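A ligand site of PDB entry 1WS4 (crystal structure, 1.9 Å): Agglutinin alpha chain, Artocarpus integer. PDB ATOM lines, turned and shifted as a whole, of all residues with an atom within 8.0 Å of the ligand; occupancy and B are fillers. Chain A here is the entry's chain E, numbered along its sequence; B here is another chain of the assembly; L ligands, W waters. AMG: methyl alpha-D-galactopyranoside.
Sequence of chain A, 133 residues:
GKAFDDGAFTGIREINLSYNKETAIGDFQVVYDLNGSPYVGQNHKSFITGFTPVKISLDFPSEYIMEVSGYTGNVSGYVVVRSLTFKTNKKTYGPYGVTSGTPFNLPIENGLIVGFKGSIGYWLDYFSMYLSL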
ATOM      1  N   GLY A   1      11.826  26.847  17.524  1.00  0.00           N
ATOM      2  CA  GLY A   1      13.008  26.956  18.419  1.00  0.00           C
ATOM      3  C   GLY A   1      14.304  26.897  17.625  1.00  0.00           C
ATOM      4  O   GLY A   1      14.282  26.793  16.396  1.00  0.00           O
ATOM      5  N   LYS A   2      15.431  26.949  18.326  1.00  0.00           N
ATOM      6  CA  LYS A   2      16.733  26.888  17.668  1.00  0.00           C
ATOM      7  C   LYS A   2      17.159  25.445  17.471  1.00  0.00           C
ATOM      8  O   LYS A   2      17.319  24.689  18.433  1.00  0.00           O
ATOM      9  CB  LYS A   2      17.792  27.620  18.507  1.00  0.00           C
ATOM     10  CG  LYS A   2      19.152  27.662  17.837  1.00  0.00           C
ATOM     11  CD  LYS A   2      20.175  28.399  18.688  1.00  0.00           C
ATOM     12  CE  LYS A   2      21.533  28.431  17.984  1.00  0.00           C
ATOM     13  NZ  LYS A   2      22.593  29.020  18.851  1.00  0.00           N
ATOM     14  N   ALA A  24       7.427  21.114  30.100  1.00  0.00           N
ATOM     15  CA  ALA A  24       8.095  20.063  29.340  1.00  0.00           C
ATOM     16  C   ALA A  24       9.600  20.053  29.587  1.00  0.00           C
ATOM     17  O   ALA A  24      10.096  20.670  30.529  1.00  0.00           O
ATOM     18  CB  ALA A  24       7.823  20.270  27.859  1.00  0.00           C
ATOM     19  N   ILE A  25      10.315  19.331  28.730  1.00  0.00           N
ATOM     20  CA  ILE A  25      11.756  19.236  28.837  1.00  0.00           C
ATOM     21  C   ILE A  25      12.352  20.557  28.374  1.00  0.00           C
ATOM     22  O   ILE A  25      11.871  21.166  27.425  1.00  0.00           O
ATOM     23  CB  ILE A  25      12.277  18.097  27.971  1.00  0.00           C
ATOM     24  CG1 ILE A  25      11.739  16.784  28.518  1.00  0.00           C
ATOM     25  CG2 ILE A  25      13.806  18.119  27.917  1.00  0.00           C
ATOM     26  CD1 ILE A  25      11.876  15.639  27.560  1.00  0.00           C
ATOM     27  N   SER A  46      17.216  26.104  26.889  1.00  0.00           N
ATOM     28  CA  SER A  46      15.906  26.708  26.662  1.00  0.00           C
ATOM     29  C   SER A  46      16.056  28.231  26.678  1.00  0.00           C
ATOM     30  O   SER A  46      17.015  28.745  27.251  1.00  0.00           O
ATOM     31  CB  SER A  46      14.941  26.282  27.762  1.00  0.00           C
ATOM     32  OG  SER A  46      13.830  27.157  27.809  1.00  0.00           O
ATOM     33  N   PHE A  47      15.120  28.932  26.055  1.00  0.00           N
ATOM     34  CA  PHE A  47      15.150  30.382  26.031  1.00  0.00           C
ATOM     35  C   PHE A  47      14.786  30.948  27.410  1.00  0.00           C
ATOM     36  O   PHE A  47      14.976  32.136  27.661  1.00  0.00           O
ATOM     37  CB  PHE A  47      14.174  30.958  24.994  1.00  0.00           C
ATOM     38  CG  PHE A  47      14.509  30.609  23.577  1.00  0.00           C
ATOM     39  CD1 PHE A  47      15.804  30.275  23.191  1.00  0.00           C
ATOM     40  CD2 PHE A  47      13.518  30.648  22.595  1.00  0.00           C
ATOM     41  CE1 PHE A  47      16.113  29.986  21.864  1.00  0.00           C
ATOM     42  CE2 PHE A  47      13.815  30.360  21.263  1.00  0.00           C
ATOM     43  CZ  PHE A  47      15.116  30.023  20.898  1.00  0.00           C
ATOM     44  N   ILE A  48      14.250  30.099  28.278  1.00  0.00           N
ATOM     45  CA  ILE A  48      13.854  30.535  29.618  1.00  0.00           C
ATOM     46  C   ILE A  48      14.492  29.683  30.703  1.00  0.00           C
ATOM     47  O   ILE A  48      15.238  28.745  30.394  1.00  0.00           O
ATOM     48  CB  ILE A  48      12.322  30.497  29.789  1.00  0.00           C
ATOM     49  CG1 ILE A  48      11.801  29.076  29.517  1.00  0.00           C
ATOM     50  CG2 ILE A  48      11.671  31.489  28.835  1.00  0.00           C
ATOM     51  CD1 ILE A  48      10.309  28.924  29.701  1.00  0.00           C
ATOM     52  N   VAL A  75       1.768  22.435  24.657  1.00  0.00           N
ATOM     53  CA  VAL A  75       2.053  23.319  25.770  1.00  0.00           C
ATOM     54  C   VAL A  75       2.074  24.707  25.136  1.00  0.00           C
ATOM     55  O   VAL A  75       2.846  24.960  24.219  1.00  0.00           O
ATOM     56  CB  VAL A  75       3.434  23.050  26.428  1.00  0.00           C
ATOM     57  CG1 VAL A  75       3.662  24.064  27.538  1.00  0.00           C
ATOM     58  CG2 VAL A  75       3.484  21.635  26.996  1.00  0.00           C
ATOM     59  N   SER A  76       1.189  25.581  25.609  1.00  0.00           N
ATOM     60  CA  SER A  76       1.106  26.947  25.093  1.00  0.00           C
ATOM     61  C   SER A  76       0.883  27.028  23.582  1.00  0.00           C
ATOM     62  O   SER A  76       1.362  27.954  22.923  1.00  0.00           O
ATOM     63  CB  SER A  76       2.387  27.710  25.464  1.00  0.00           C
ATOM     64  OG  SER A  76       2.271  29.077  25.126  1.00  0.00           O
ATOM     65  N   GLY A  77       0.153  26.067  23.024  1.00  0.00           N
ATOM     66  CA  GLY A  77      -0.116  26.092  21.597  1.00  0.00           C
ATOM     67  C   GLY A  77       0.965  25.493  20.708  1.00  0.00           C
ATOM     68  O   GLY A  77       0.863  25.562  19.481  1.00  0.00           O
ATOM     69  N   TYR A  78       1.991  24.920  21.320  1.00  0.00           N
ATOM     70  CA  TYR A  78       3.091  24.301  20.589  1.00  0.00           C
ATOM     71  C   TYR A  78       3.156  22.810  20.918  1.00  0.00           C
ATOM     72  O   TYR A  78       2.836  22.409  22.033  1.00  0.00           O
ATOM     73  CB  TYR A  78       4.448  24.896  21.008  1.00  0.00           C
ATOM     74  CG  TYR A  78       4.572  26.396  20.893  1.00  0.00           C
ATOM     75  CD1 TYR A  78       4.849  27.013  19.678  1.00  0.00           C
ATOM     76  CD2 TYR A  78       4.446  27.197  22.027  1.00  0.00           C
ATOM     77  CE1 TYR A  78       4.993  28.395  19.586  1.00  0.00           C
ATOM     78  CE2 TYR A  78       4.593  28.581  21.949  1.00  0.00           C
ATOM     79  CZ  TYR A  78       4.861  29.169  20.730  1.00  0.00           C
ATOM     80  OH  TYR A  78       5.021  30.536  20.674  1.00  0.00           O
ATOM     81  N   VAL A  79       3.565  21.994  19.951  1.00  0.00           N
ATOM     82  CA  VAL A  79       3.717  20.572  20.210  1.00  0.00           C
ATOM     83  C   VAL A  79       5.181  20.399  20.624  1.00  0.00           C
ATOM     84  O   VAL A  79       6.091  20.760  19.876  1.00  0.00           O
ATOM     85  CB  VAL A  79       3.449  19.711  18.963  1.00  0.00           C
ATOM     86  CG1 VAL A  79       3.703  18.249  19.282  1.00  0.00           C
ATOM     87  CG2 VAL A  79       2.002  19.901  18.509  1.00  0.00           C
ATOM     88  N   VAL A  80       5.401  19.855  21.814  1.00  0.00           N
ATOM     89  CA  VAL A  80       6.758  19.658  22.318  1.00  0.00           C
ATOM     90  C   VAL A  80       6.922  18.314  23.013  1.00  0.00           C
ATOM     91  O   VAL A  80       5.963  17.573  23.209  1.00  0.00           O
ATOM     92  CB  VAL A  80       7.127  20.777  23.324  1.00  0.00           C
ATOM     93  CG1 VAL A  80       7.111  22.129  22.642  1.00  0.00           C
ATOM     94  CG2 VAL A  80       6.166  20.765  24.505  1.00  0.00           C
ATOM     95  N   VAL A  81       8.160  18.011  23.394  1.00  0.00           N
ATOM     96  CA  VAL A  81       8.468  16.768  24.093  1.00  0.00           C
ATOM     97  C   VAL A  81       8.279  17.085  25.578  1.00  0.00           C
ATOM     98  O   VAL A  81       9.038  17.868  26.149  1.00  0.00           O
ATOM     99  CB  VAL A  81       9.913  16.309  23.840  1.00  0.00           C
ATOM    100  CG1 VAL A  81      10.203  15.042  24.617  1.00  0.00           C
ATOM    101  CG2 VAL A  81      10.132  16.089  22.356  1.00  0.00           C
ATOM    102  N   SER A 119      15.533  20.430  18.328  1.00  0.00           N
ATOM    103  CA  SER A 119      15.288  21.863  18.376  1.00  0.00           C
ATOM    104  C   SER A 119      14.763  22.247  19.740  1.00  0.00           C
ATOM    105  O   SER A 119      13.986  21.513  20.339  1.00  0.00           O
ATOM    106  CB  SER A 119      14.259  22.242  17.302  1.00  0.00           C
ATOM    107  OG  SER A 119      13.949  23.625  17.351  1.00  0.00           O
ATOM    108  N   ILE A 120      15.208  23.399  20.243  1.00  0.00           N
ATOM    109  CA  ILE A 120      14.753  23.867  21.545  1.00  0.00           C
ATOM    110  C   ILE A 120      14.434  25.363  21.505  1.00  0.00           C
ATOM    111  O   ILE A 120      15.247  26.166  21.038  1.00  0.00           O
ATOM    112  CB  ILE A 120      15.819  23.645  22.648  1.00  0.00           C
ATOM    113  CG1 ILE A 120      16.169  22.157  22.748  1.00  0.00           C
ATOM    114  CG2 ILE A 120      15.292  24.155  23.986  1.00  0.00           C
ATOM    115  CD1 ILE A 120      17.280  21.853  23.744  1.00  0.00           C
ATOM    116  N   GLY A 121      13.244  25.705  21.976  1.00  0.00           N
ATOM    117  CA  GLY A 121      12.822  27.093  22.055  1.00  0.00           C
ATOM    118  C   GLY A 121      12.650  27.251  23.546  1.00  0.00           C
ATOM    119  O   GLY A 121      13.627  27.231  24.284  1.00  0.00           O
ATOM    120  N   TYR A 122      11.414  27.400  24.020  1.00  0.00           N
ATOM    121  CA  TYR A 122      11.189  27.463  25.456  1.00  0.00           C
ATOM    122  C   TYR A 122      11.381  26.027  25.934  1.00  0.00           C
ATOM    123  O   TYR A 122      11.852  25.784  27.050  1.00  0.00           O
ATOM    124  CB  TYR A 122       9.765  27.911  25.786  1.00  0.00           C
ATOM    125  CG  TYR A 122       9.563  29.407  25.815  1.00  0.00           C
ATOM    126  CD1 TYR A 122       8.520  29.969  26.565  1.00  0.00           C
ATOM    127  CD2 TYR A 122      10.387  30.269  25.103  1.00  0.00           C
ATOM    128  CE1 TYR A 122       8.321  31.355  26.604  1.00  0.00           C
ATOM    129  CE2 TYR A 122      10.200  31.652  25.133  1.00  0.00           C
ATOM    130  CZ  TYR A 122       9.157  32.190  25.878  1.00  0.00           C
ATOM    131  OH  TYR A 122       8.961  33.545  25.905  1.00  0.00           O
ATOM    132  N   TRP A 123      10.994  25.084  25.078  1.00  0.00           N
ATOM    133  CA  TRP A 123      11.100  23.663  25.394  1.00  0.00           C
ATOM    134  C   TRP A 123      11.654  22.881  24.208  1.00  0.00           C
ATOM    135  O   TRP A 123      11.843  23.429  23.121  1.00  0.00           O
ATOM    136  CB  TRP A 123       9.713  23.121  25.758  1.00  0.00           C
ATOM    137  CG  TRP A 123       9.053  23.917  26.851  1.00  0.00           C
ATOM    138  CD1 TRP A 123       9.419  23.966  28.163  1.00  0.00           C
ATOM    139  CD2 TRP A 123       7.969  24.843  26.709  1.00  0.00           C
ATOM    140  NE1 TRP A 123       8.642  24.869  28.846  1.00  0.00           N
ATOM    141  CE2 TRP A 123       7.744  25.425  27.973  1.00  0.00           C
ATOM    142  CE3 TRP A 123       7.167  25.246  25.627  1.00  0.00           C
ATOM    143  CZ2 TRP A 123       6.748  26.387  28.188  1.00  0.00           C
ATOM    144  CZ3 TRP A 123       6.184  26.208  25.848  1.00  0.00           C
ATOM    145  CH2 TRP A 123       5.976  26.760  27.119  1.00  0.00           C
ATOM    146  N   LEU A 124      11.937  21.609  24.433  1.00  0.00           N
ATOM    147  CA  LEU A 124      12.443  20.731  23.386  1.00  0.00           C
ATOM    148  C   LEU A 124      11.293  20.510  22.410  1.00  0.00           C
ATOM    149  O   LEU A 124      10.320  19.819  22.726  1.00  0.00           O
ATOM    150  CB  LEU A 124      12.876  19.394  24.004  1.00  0.00           C
ATOM    151  CG  LEU A 124      13.455  18.317  23.080  1.00  0.00           C
ATOM    152  CD1 LEU A 124      14.785  18.777  22.503  1.00  0.00           C
ATOM    153  CD2 LEU A 124      13.634  17.022  23.861  1.00  0.00           C
ATOM    154  N   ASP A 125      11.391  21.104  21.217  1.00  0.00           N
ATOM    155  CA  ASP A 125      10.353  20.998  20.192  1.00  0.00           C
ATOM    156  C   ASP A 125      10.236  19.595  19.628  1.00  0.00           C
ATOM    157  O   ASP A 125       9.137  19.077  19.435  1.00  0.00           O
ATOM    158  CB  ASP A 125      10.642  21.967  19.048  1.00  0.00           C
ATOM    159  CG  ASP A 125      10.694  23.405  19.496  1.00  0.00           C
ATOM    160  OD1 ASP A 125       9.718  23.856  20.117  1.00  0.00           O
ATOM    161  OD2 ASP A 125      11.724  24.071  19.225  1.00  0.00           O
ATOM    162  N   TYR A 126      11.386  19.002  19.324  1.00  0.00           N
ATOM    163  CA  TYR A 126      11.423  17.657  18.767  1.00  0.00           C
ATOM    164  C   TYR A 126      12.874  17.190  18.801  1.00  0.00           C
ATOM    165  O   TYR A 126      13.785  17.992  18.981  1.00  0.00           O
ATOM    166  CB  TYR A 126      10.923  17.655  17.320  1.00  0.00           C
ATOM    167  CG  TYR A 126      11.720  18.546  16.380  1.00  0.00           C
ATOM    168  CD1 TYR A 126      12.976  18.143  15.905  1.00  0.00           C
ATOM    169  CD2 TYR A 126      11.224  19.781  15.975  1.00  0.00           C
ATOM    170  CE1 TYR A 126      13.715  18.980  15.044  1.00  0.00           C
ATOM    171  CE2 TYR A 126      11.949  20.604  15.124  1.00  0.00           C
ATOM    172  CZ  TYR A 126      13.186  20.198  14.661  1.00  0.00           C
ATOM    173  OH  TYR A 126      13.897  21.029  13.825  1.00  0.00           O
ATOM    174  N   ALA B  17       7.217  18.116  17.549  1.00  0.00           N
ATOM    175  CA  ALA B  17       6.625  18.937  16.495  1.00  0.00           C
ATOM    176  C   ALA B  17       6.922  18.312  15.139  1.00  0.00           C
ATOM    177  O   ALA B  17       7.979  17.718  14.936  1.00  0.00           O
ATOM    178  CB  ALA B  17       7.174  20.354  16.561  1.00  0.00           C
HETATM  179  C1  AMG L   1       9.368  29.580  21.682  1.00  0.00           C
HETATM  180  C2  AMG L   1       9.901  29.496  20.237  1.00  0.00           C
HETATM  181  C3  AMG L   1       9.017  28.592  19.353  1.00  0.00           C
HETATM  182  C4  AMG L   1       8.990  27.193  19.982  1.00  0.00           C
HETATM  183  C5  AMG L   1       8.406  27.298  21.403  1.00  0.00           C
HETATM  184  C6  AMG L   1       8.333  25.923  22.094  1.00  0.00           C
HETATM  185  C7  AMG L   1       7.558  30.448  23.079  1.00  0.00           C
HETATM  186  O1  AMG L   1       8.106  30.310  21.737  1.00  0.00           O
HETATM  187  O2  AMG L   1       9.986  30.814  19.679  1.00  0.00           O
HETATM  188  O3  AMG L   1       9.571  28.529  18.010  1.00  0.00           O
HETATM  189  O4  AMG L   1      10.201  26.562  19.824  1.00  0.00           O
HETATM  190  O5  AMG L   1       9.228  28.207  22.218  1.00  0.00           O
HETATM  191  O6  AMG L   1       9.643  25.441  22.417  1.00  0.00           O
HETATM  192  O   HOH W   1      11.020  33.249  21.506  1.00  0.00           O
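O4 of the ligand sits at hydrogen-bond distance from OD1 of Asp 125 (2.8 Å). The backbone NH (N) of Gly 1 is in hydrogen-bond range of an oxygen (O4) of the ligand. The backbone NH (N) of Tyr 122 lies within hydrogen-bond range of an oxygen (O5) of the ligand (2.9 Å). The backbone NH (N) of Trp 123 is in hydrogen-bond range of an oxygen (O6) of the ligand, at 3.0 Å. The backbone carbonyl oxygen (O) of Trp 123 is in hydrogen-bond range of an oxygen (O6) of the ligand, 3.1 Å away. An oxygen (O1) of the ligand is in hydrogen-bond range of the side-chain hydroxyl of Tyr 78 (3.3 Å).
Gly 121 touches the ligand (CA to O4, 3.5 Å). Hydrophobic or aromatic side chains that line the ligand: Tyr 78, Tyr 122 and Trp 123. Of the 23 residues printed, 6 come within 4 Å of the ligand.
N of Gly 1 sits at hydrogen-bond distance from OD2 of Asp 125. The backbone NH of Asp 125 is in hydrogen-bond range of the backbone carbonyl oxygen of Ser 119 (2.8 Å). The backbone carbonyl oxygen (O) of Asp 125 lies within hydrogen-bond range of the backbone NH (N) of Ala 17 of chain B. O of Gly 1 sits close to OG of Ser 119 (3.3 Å). O of Tyr 122 lies within hydrogen-bond range of OG of Ser 46 (2.5 Å). The backbone carbonyl oxygen (O) of Gly 121 lies within hydrogen-bond range of the backbone NH (N) of Phe 47 (2.9 Å).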
